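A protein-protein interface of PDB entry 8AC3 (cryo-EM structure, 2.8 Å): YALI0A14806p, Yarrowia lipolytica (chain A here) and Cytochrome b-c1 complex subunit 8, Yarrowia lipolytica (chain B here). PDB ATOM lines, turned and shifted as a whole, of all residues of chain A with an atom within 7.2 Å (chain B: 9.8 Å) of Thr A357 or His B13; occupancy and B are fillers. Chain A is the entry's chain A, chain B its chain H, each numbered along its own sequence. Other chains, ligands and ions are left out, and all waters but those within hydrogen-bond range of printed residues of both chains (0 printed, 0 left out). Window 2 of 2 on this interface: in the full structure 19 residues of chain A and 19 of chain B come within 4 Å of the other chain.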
ATOM      1  N   SER A 353     -17.746   6.067  19.910  1.00  0.00           N
ATOM      2  CA  SER A 353     -17.354   4.677  19.936  1.00  0.00           C
ATOM      3  C   SER A 353     -18.227   3.902  18.970  1.00  0.00           C
ATOM      4  O   SER A 353     -19.438   4.094  18.959  1.00  0.00           O
ATOM      5  CB  SER A 353     -17.505   4.126  21.323  1.00  0.00           C
ATOM      6  OG  SER A 353     -17.203   2.739  21.336  1.00  0.00           O
ATOM      7  N   GLU A 354     -17.600   2.975  18.236  1.00  0.00           N
ATOM      8  CA  GLU A 354     -18.332   1.986  17.465  1.00  0.00           C
ATOM      9  C   GLU A 354     -18.429   0.664  18.219  1.00  0.00           C
ATOM     10  O   GLU A 354     -19.031  -0.285  17.727  1.00  0.00           O
ATOM     11  CB  GLU A 354     -17.600   1.671  16.168  1.00  0.00           C
ATOM     12  CG  GLU A 354     -17.517   2.839  15.211  1.00  0.00           C
ATOM     13  CD  GLU A 354     -16.325   2.861  14.256  1.00  0.00           C
ATOM     14  OE1 GLU A 354     -16.324   3.708  13.324  1.00  0.00           O
ATOM     15  OE2 GLU A 354     -15.379   2.051  14.444  1.00  0.00           O
ATOM     16  N   ASN A 355     -17.784   0.571  19.378  1.00  0.00           N
ATOM     17  CA  ASN A 355     -17.702  -0.699  20.068  1.00  0.00           C
ATOM     18  C   ASN A 355     -18.937  -0.806  20.943  1.00  0.00           C
ATOM     19  O   ASN A 355     -18.895  -0.499  22.128  1.00  0.00           O
ATOM     20  CB  ASN A 355     -16.401  -0.785  20.859  1.00  0.00           C
ATOM     21  CG  ASN A 355     -16.119  -2.129  21.502  1.00  0.00           C
ATOM     22  OD1 ASN A 355     -16.985  -3.001  21.584  1.00  0.00           O
ATOM     23  ND2 ASN A 355     -14.890  -2.303  21.963  1.00  0.00           N
ATOM     24  N   THR A 356     -20.034  -1.253  20.357  1.00  0.00           N
ATOM     25  CA  THR A 356     -21.300  -1.024  21.027  1.00  0.00           C
ATOM     26  C   THR A 356     -21.556  -2.042  22.134  1.00  0.00           C
ATOM     27  O   THR A 356     -22.429  -1.832  22.967  1.00  0.00           O
ATOM     28  CB  THR A 356     -22.435  -0.939  20.014  1.00  0.00           C
ATOM     29  OG1 THR A 356     -22.371  -2.145  19.254  1.00  0.00           O
ATOM     30  CG2 THR A 356     -22.296   0.285  19.139  1.00  0.00           C
ATOM     31  N   THR A 357     -20.775  -3.119  22.158  1.00  0.00           N
ATOM     32  CA  THR A 357     -20.907  -4.102  23.217  1.00  0.00           C
ATOM     33  C   THR A 357     -19.979  -3.787  24.390  1.00  0.00           C
ATOM     34  O   THR A 357     -19.984  -4.504  25.387  1.00  0.00           O
ATOM     35  CB  THR A 357     -20.668  -5.503  22.658  1.00  0.00           C
ATOM     36  OG1 THR A 357     -19.308  -5.516  22.220  1.00  0.00           O
ATOM     37  CG2 THR A 357     -21.607  -5.817  21.513  1.00  0.00           C
ATOM     38  N   GLN A 358     -19.160  -2.740  24.285  1.00  0.00           N
ATOM     39  CA  GLN A 358     -18.295  -2.458  25.416  1.00  0.00           C
ATOM     40  C   GLN A 358     -18.414  -1.005  25.832  1.00  0.00           C
ATOM     41  O   GLN A 358     -17.493  -0.442  26.421  1.00  0.00           O
ATOM     42  CB  GLN A 358     -16.861  -2.815  25.077  1.00  0.00           C
ATOM     43  CG  GLN A 358     -16.596  -4.305  25.063  1.00  0.00           C
ATOM     44  CD  GLN A 358     -15.100  -4.462  24.995  1.00  0.00           C
ATOM     45  OE1 GLN A 358     -14.526  -4.594  23.914  1.00  0.00           O
ATOM     46  NE2 GLN A 358     -14.454  -4.395  26.153  1.00  0.00           N
ATOM     47  N   ILE A 359     -19.578  -0.425  25.571  1.00  0.00           N
ATOM     48  CA  ILE A 359     -19.816   0.941  25.994  1.00  0.00           C
ATOM     49  C   ILE A 359     -19.747   1.016  27.515  1.00  0.00           C
ATOM     50  O   ILE A 359     -19.250   1.996  28.073  1.00  0.00           O
ATOM     51  CB  ILE A 359     -21.168   1.402  25.455  1.00  0.00           C
ATOM     52  CG1 ILE A 359     -21.007   1.861  24.013  1.00  0.00           C
ATOM     53  CG2 ILE A 359     -21.785   2.484  26.324  1.00  0.00           C
ATOM     54  CD1 ILE A 359     -22.339   2.068  23.394  1.00  0.00           C
ATOM     55  N   ASP A 360     -20.228  -0.047  28.166  1.00  0.00           N
ATOM     56  CA  ASP A 360     -20.205  -0.117  29.611  1.00  0.00           C
ATOM     57  C   ASP A 360     -18.769   0.007  30.103  1.00  0.00           C
ATOM     58  O   ASP A 360     -18.532   0.762  31.040  1.00  0.00           O
ATOM     59  CB  ASP A 360     -20.904  -1.367  30.135  1.00  0.00           C
ATOM     60  CG  ASP A 360     -20.281  -2.684  29.707  1.00  0.00           C
ATOM     61  OD1 ASP A 360     -19.723  -2.748  28.590  1.00  0.00           O
ATOM     62  OD2 ASP A 360     -20.380  -3.647  30.495  1.00  0.00           O
ATOM     63  N   ASP A 361     -17.828  -0.673  29.433  1.00  0.00           N
ATOM     64  CA  ASP A 361     -16.430  -0.626  29.829  1.00  0.00           C
ATOM     65  C   ASP A 361     -15.871   0.768  29.610  1.00  0.00           C
ATOM     66  O   ASP A 361     -15.195   1.315  30.481  1.00  0.00           O
ATOM     67  CB  ASP A 361     -15.594  -1.675  29.105  1.00  0.00           C
ATOM     68  CG  ASP A 361     -15.996  -3.094  29.472  1.00  0.00           C
ATOM     69  OD1 ASP A 361     -16.143  -3.379  30.686  1.00  0.00           O
ATOM     70  OD2 ASP A 361     -16.173  -3.903  28.544  1.00  0.00           O
ATOM     71  N   PRO A 455     -26.400   4.018  18.978  1.00  0.00           N
ATOM     72  CA  PRO A 455     -26.627   2.674  19.500  1.00  0.00           C
ATOM     73  C   PRO A 455     -26.108   2.541  20.929  1.00  0.00           C
ATOM     74  O   PRO A 455     -25.039   1.986  21.161  1.00  0.00           O
ATOM     75  CB  PRO A 455     -25.845   1.858  18.478  1.00  0.00           C
ATOM     76  CG  PRO A 455     -24.675   2.743  18.153  1.00  0.00           C
ATOM     77  CD  PRO A 455     -25.260   4.129  18.058  1.00  0.00           C
ATOM     78  N   GLU A 457     -27.719   1.002  23.529  1.00  0.00           N
ATOM     79  CA  GLU A 457     -28.377  -0.060  24.279  1.00  0.00           C
ATOM     80  C   GLU A 457     -27.514  -0.502  25.456  1.00  0.00           C
ATOM     81  O   GLU A 457     -28.031  -0.760  26.541  1.00  0.00           O
ATOM     82  CB  GLU A 457     -28.657  -1.272  23.394  1.00  0.00           C
ATOM     83  CG  GLU A 457     -29.365  -2.393  24.129  1.00  0.00           C
ATOM     84  CD  GLU A 457     -29.606  -3.628  23.282  1.00  0.00           C
ATOM     85  OE1 GLU A 457     -30.603  -3.662  22.518  1.00  0.00           O
ATOM     86  OE2 GLU A 457     -28.788  -4.553  23.390  1.00  0.00           O
ATOM     87  N   GLY A 458     -26.202  -0.570  25.232  1.00  0.00           N
ATOM     88  CA  GLY A 458     -25.291  -1.068  26.241  1.00  0.00           C
ATOM     89  C   GLY A 458     -24.919  -0.028  27.293  1.00  0.00           C
ATOM     90  O   GLY A 458     -24.125  -0.325  28.182  1.00  0.00           O
ATOM     91  N   TYR B   7     -33.239 -15.920  22.192  1.00  0.00           N
ATOM     92  CA  TYR B   7     -34.469 -14.988  22.418  1.00  0.00           C
ATOM     93  C   TYR B   7     -34.195 -13.798  23.334  1.00  0.00           C
ATOM     94  O   TYR B   7     -34.969 -12.834  23.377  1.00  0.00           O
ATOM     95  CB  TYR B   7     -35.685 -15.726  22.987  1.00  0.00           C
ATOM     96  CG  TYR B   7     -36.425 -16.555  21.973  1.00  0.00           C
ATOM     97  CD1 TYR B   7     -36.960 -15.992  20.819  1.00  0.00           C
ATOM     98  CD2 TYR B   7     -36.554 -17.923  22.151  1.00  0.00           C
ATOM     99  CE1 TYR B   7     -37.598 -16.769  19.864  1.00  0.00           C
ATOM    100  CE2 TYR B   7     -37.202 -18.712  21.213  1.00  0.00           C
ATOM    101  CZ  TYR B   7     -37.728 -18.135  20.067  1.00  0.00           C
ATOM    102  OH  TYR B   7     -38.368 -18.912  19.144  1.00  0.00           O
ATOM    103  N   MET B   8     -33.143 -13.891  24.138  1.00  0.00           N
ATOM    104  CA  MET B   8     -32.629 -12.708  24.793  1.00  0.00           C
ATOM    105  C   MET B   8     -31.134 -12.663  24.520  1.00  0.00           C
ATOM    106  O   MET B   8     -30.460 -13.687  24.607  1.00  0.00           O
ATOM    107  CB  MET B   8     -32.883 -12.745  26.297  1.00  0.00           C
ATOM    108  CG  MET B   8     -32.381 -11.491  26.961  1.00  0.00           C
ATOM    109  SD  MET B   8     -32.478 -11.524  28.754  1.00  0.00           S
ATOM    110  CE  MET B   8     -31.298 -12.811  29.173  1.00  0.00           C
ATOM    111  N   GLY B   9     -30.614 -11.474  24.203  1.00  0.00           N
ATOM    112  CA  GLY B   9     -29.178 -11.374  24.046  1.00  0.00           C
ATOM    113  C   GLY B   9     -28.517 -10.879  25.323  1.00  0.00           C
ATOM    114  O   GLY B   9     -28.703 -11.414  26.417  1.00  0.00           O
ATOM    115  N   TRP B  10     -27.717  -9.840  25.152  1.00  0.00           N
ATOM    116  CA  TRP B  10     -27.003  -9.237  26.252  1.00  0.00           C
ATOM    117  C   TRP B  10     -26.860  -7.762  25.925  1.00  0.00           C
ATOM    118  O   TRP B  10     -27.271  -7.345  24.850  1.00  0.00           O
ATOM    119  CB  TRP B  10     -25.655  -9.923  26.441  1.00  0.00           C
ATOM    120  CG  TRP B  10     -25.133  -9.740  27.831  1.00  0.00           C
ATOM    121  CD1 TRP B  10     -24.133  -8.903  28.249  1.00  0.00           C
ATOM    122  CD2 TRP B  10     -25.649 -10.373  29.016  1.00  0.00           C
ATOM    123  NE1 TRP B  10     -23.960  -9.011  29.607  1.00  0.00           N
ATOM    124  CE2 TRP B  10     -24.874  -9.905  30.107  1.00  0.00           C
ATOM    125  CE3 TRP B  10     -26.682 -11.294  29.254  1.00  0.00           C
ATOM    126  CZ2 TRP B  10     -25.102 -10.336  31.417  1.00  0.00           C
ATOM    127  CZ3 TRP B  10     -26.884 -11.743  30.546  1.00  0.00           C
ATOM    128  CH2 TRP B  10     -26.112 -11.259  31.612  1.00  0.00           C
ATOM    129  N   TRP B  11     -26.354  -6.976  26.869  1.00  0.00           N
ATOM    130  CA  TRP B  11     -26.282  -5.545  26.636  1.00  0.00           C
ATOM    131  C   TRP B  11     -25.506  -5.265  25.359  1.00  0.00           C
ATOM    132  O   TRP B  11     -24.410  -5.781  25.152  1.00  0.00           O
ATOM    133  CB  TRP B  11     -25.568  -4.893  27.799  1.00  0.00           C
ATOM    134  CG  TRP B  11     -26.235  -5.195  29.091  1.00  0.00           C
ATOM    135  CD1 TRP B  11     -25.845  -6.101  30.031  1.00  0.00           C
ATOM    136  CD2 TRP B  11     -27.439  -4.586  29.570  1.00  0.00           C
ATOM    137  NE1 TRP B  11     -26.718  -6.074  31.083  1.00  0.00           N
ATOM    138  CE2 TRP B  11     -27.710  -5.167  30.826  1.00  0.00           C
ATOM    139  CE3 TRP B  11     -28.314  -3.623  29.051  1.00  0.00           C
ATOM    140  CZ2 TRP B  11     -28.821  -4.799  31.581  1.00  0.00           C
ATOM    141  CZ3 TRP B  11     -29.416  -3.264  29.799  1.00  0.00           C
ATOM    142  CH2 TRP B  11     -29.661  -3.845  31.044  1.00  0.00           C
ATOM    143  N   GLY B  12     -26.085  -4.426  24.516  1.00  0.00           N
ATOM    144  CA  GLY B  12     -25.470  -4.163  23.233  1.00  0.00           C
ATOM    145  C   GLY B  12     -26.164  -4.928  22.116  1.00  0.00           C
ATOM    146  O   GLY B  12     -26.254  -4.410  21.006  1.00  0.00           O
ATOM    147  N   HIS B  13     -26.661  -6.136  22.412  1.00  0.00           N
ATOM    148  CA  HIS B  13     -27.324  -6.925  21.387  1.00  0.00           C
ATOM    149  C   HIS B  13     -28.488  -7.697  22.003  1.00  0.00           C
ATOM    150  O   HIS B  13     -28.560  -8.921  21.905  1.00  0.00           O
ATOM    151  CB  HIS B  13     -26.282  -7.782  20.649  1.00  0.00           C
ATOM    152  CG  HIS B  13     -25.561  -8.716  21.560  1.00  0.00           C
ATOM    153  ND1 HIS B  13     -24.560  -8.290  22.414  1.00  0.00           N
ATOM    154  CD2 HIS B  13     -25.716 -10.041  21.782  1.00  0.00           C
ATOM    155  CE1 HIS B  13     -24.117  -9.315  23.115  1.00  0.00           C
ATOM    156  NE2 HIS B  13     -24.815 -10.403  22.750  1.00  0.00           N
ATOM    157  N   MET B  14     -29.402  -6.961  22.633  1.00  0.00           N
ATOM    158  CA  MET B  14     -30.424  -7.567  23.465  1.00  0.00           C
ATOM    159  C   MET B  14     -31.450  -8.295  22.601  1.00  0.00           C
ATOM    160  O   MET B  14     -32.052  -9.264  23.053  1.00  0.00           O
ATOM    161  CB  MET B  14     -31.156  -6.508  24.289  1.00  0.00           C
ATOM    162  CG  MET B  14     -31.897  -7.078  25.483  1.00  0.00           C
ATOM    163  SD  MET B  14     -30.738  -7.751  26.699  1.00  0.00           S
ATOM    164  CE  MET B  14     -29.913  -6.235  27.175  1.00  0.00           C
ATOM    165  N   GLY B  15     -31.641  -7.847  21.359  1.00  0.00           N
ATOM    166  CA  GLY B  15     -32.592  -8.515  20.489  1.00  0.00           C
ATOM    167  C   GLY B  15     -33.885  -7.713  20.336  1.00  0.00           C
ATOM    168  O   GLY B  15     -34.911  -8.238  19.903  1.00  0.00           O
ATOM    169  N   SER B  16     -33.807  -6.424  20.677  1.00  0.00           N
ATOM    170  CA  SER B  16     -34.856  -5.469  20.375  1.00  0.00           C
ATOM    171  C   SER B  16     -34.960  -5.302  18.860  1.00  0.00           C
ATOM    172  O   SER B  16     -33.951  -5.368  18.153  1.00  0.00           O
ATOM    173  CB  SER B  16     -34.560  -4.162  21.057  1.00  0.00           C
ATOM    174  OG  SER B  16     -35.498  -3.160  20.696  1.00  0.00           O
ATOM    175  N   PRO B  17     -36.172  -5.071  18.309  1.00  0.00           N
ATOM    176  CA  PRO B  17     -36.293  -4.511  16.963  1.00  0.00           C
ATOM    177  C   PRO B  17     -35.545  -3.184  16.992  1.00  0.00           C
ATOM    178  O   PRO B  17     -35.386  -2.591  18.057  1.00  0.00           O
ATOM    179  CB  PRO B  17     -37.776  -4.169  16.882  1.00  0.00           C
ATOM    180  CG  PRO B  17     -38.424  -5.163  17.798  1.00  0.00           C
ATOM    181  CD  PRO B  17     -37.468  -5.313  18.955  1.00  0.00           C
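Of the printed residues of chain B, Thr A357 touches His B13.
Thr A356 touches just one residue of chain B: Gly B12.
No residue of chain B comes within 4 Å of Gln A358.
Of chain A, only Thr A356, Glu A457 and Gly A458 come within 4 Å of Gly B12.
Of the printed residues of chain B, Glu A457 touches Trp B10 (3.5 Å), Trp B11 (3.8 Å), Gly B12 (2.9 Å), His B13 (2.8 Å) and Met B14 (2.6 Å).
Of the printed residues of chain A, Trp B11 touches Glu A457 (3.8 Å).
Of the printed residues of chain B, Gly A458 touches Gly B12.
Of the printed residues of chain A, Trp B10 touches Glu A457 (3.5 Å).
Printed residues of chain A within 4 Å of Met B14: Glu A457 (2.6 Å).
The nearest residue of chain A that does not touch His B13 is Thr A356 (6.1 Å).
The nearest printed residue of chain B that does not touch Glu A457 is Ser B16 (4.2 Å).
Thr A356 touches Gly B12 (O to CA, 3.8 Å).
CG2 of Thr A357 touches ND1 of His B13, 3.96 Å away.
Trp B11 touches Glu A457 (CE3 to O, 3.8 Å).
Gly A458 touches Gly B12 (CA to N, 3.9 Å).
The side-chain hydroxyl (OG1) of Thr A357 sits at hydrogen-bond distance from the side-chain amide oxygen (OD1) of Asn A355 (3.5 Å).
N of Gly B9 lies within hydrogen-bond range of O of Met B14.
OE2 of Glu A457 sits at hydrogen-bond distance from N of His B13 (2.8 Å).
The backbone carbonyl oxygen (O) of Trp B10 lies close to the side-chain carboxylate (OE2) of Glu A457 (3.5 Å).
N of Gly B12 sits at hydrogen-bond distance from OE2 of Glu A457 (2.9 Å).
The backbone NH (N) of Met B14 sits at hydrogen-bond distance from the side-chain carboxylate (OE2) of Glu A457 (2.6 Å).
Of the 11 printed residues of chain B, 5 touch a printed residue of chain A.
Printed residues of chain B that touch a printed residue of chain A: Trp B10, Trp B11, Gly B12, His B13 and Met B14.
Hydrophobic or aromatic side chains of chain B that line the printed part of chain A: Trp B11, His B13 and Met B14.
Among the printed residues, no Asp or Glu carboxylate lies within 4 Å of a Lys or Arg side-chain nitrogen of the other chain.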
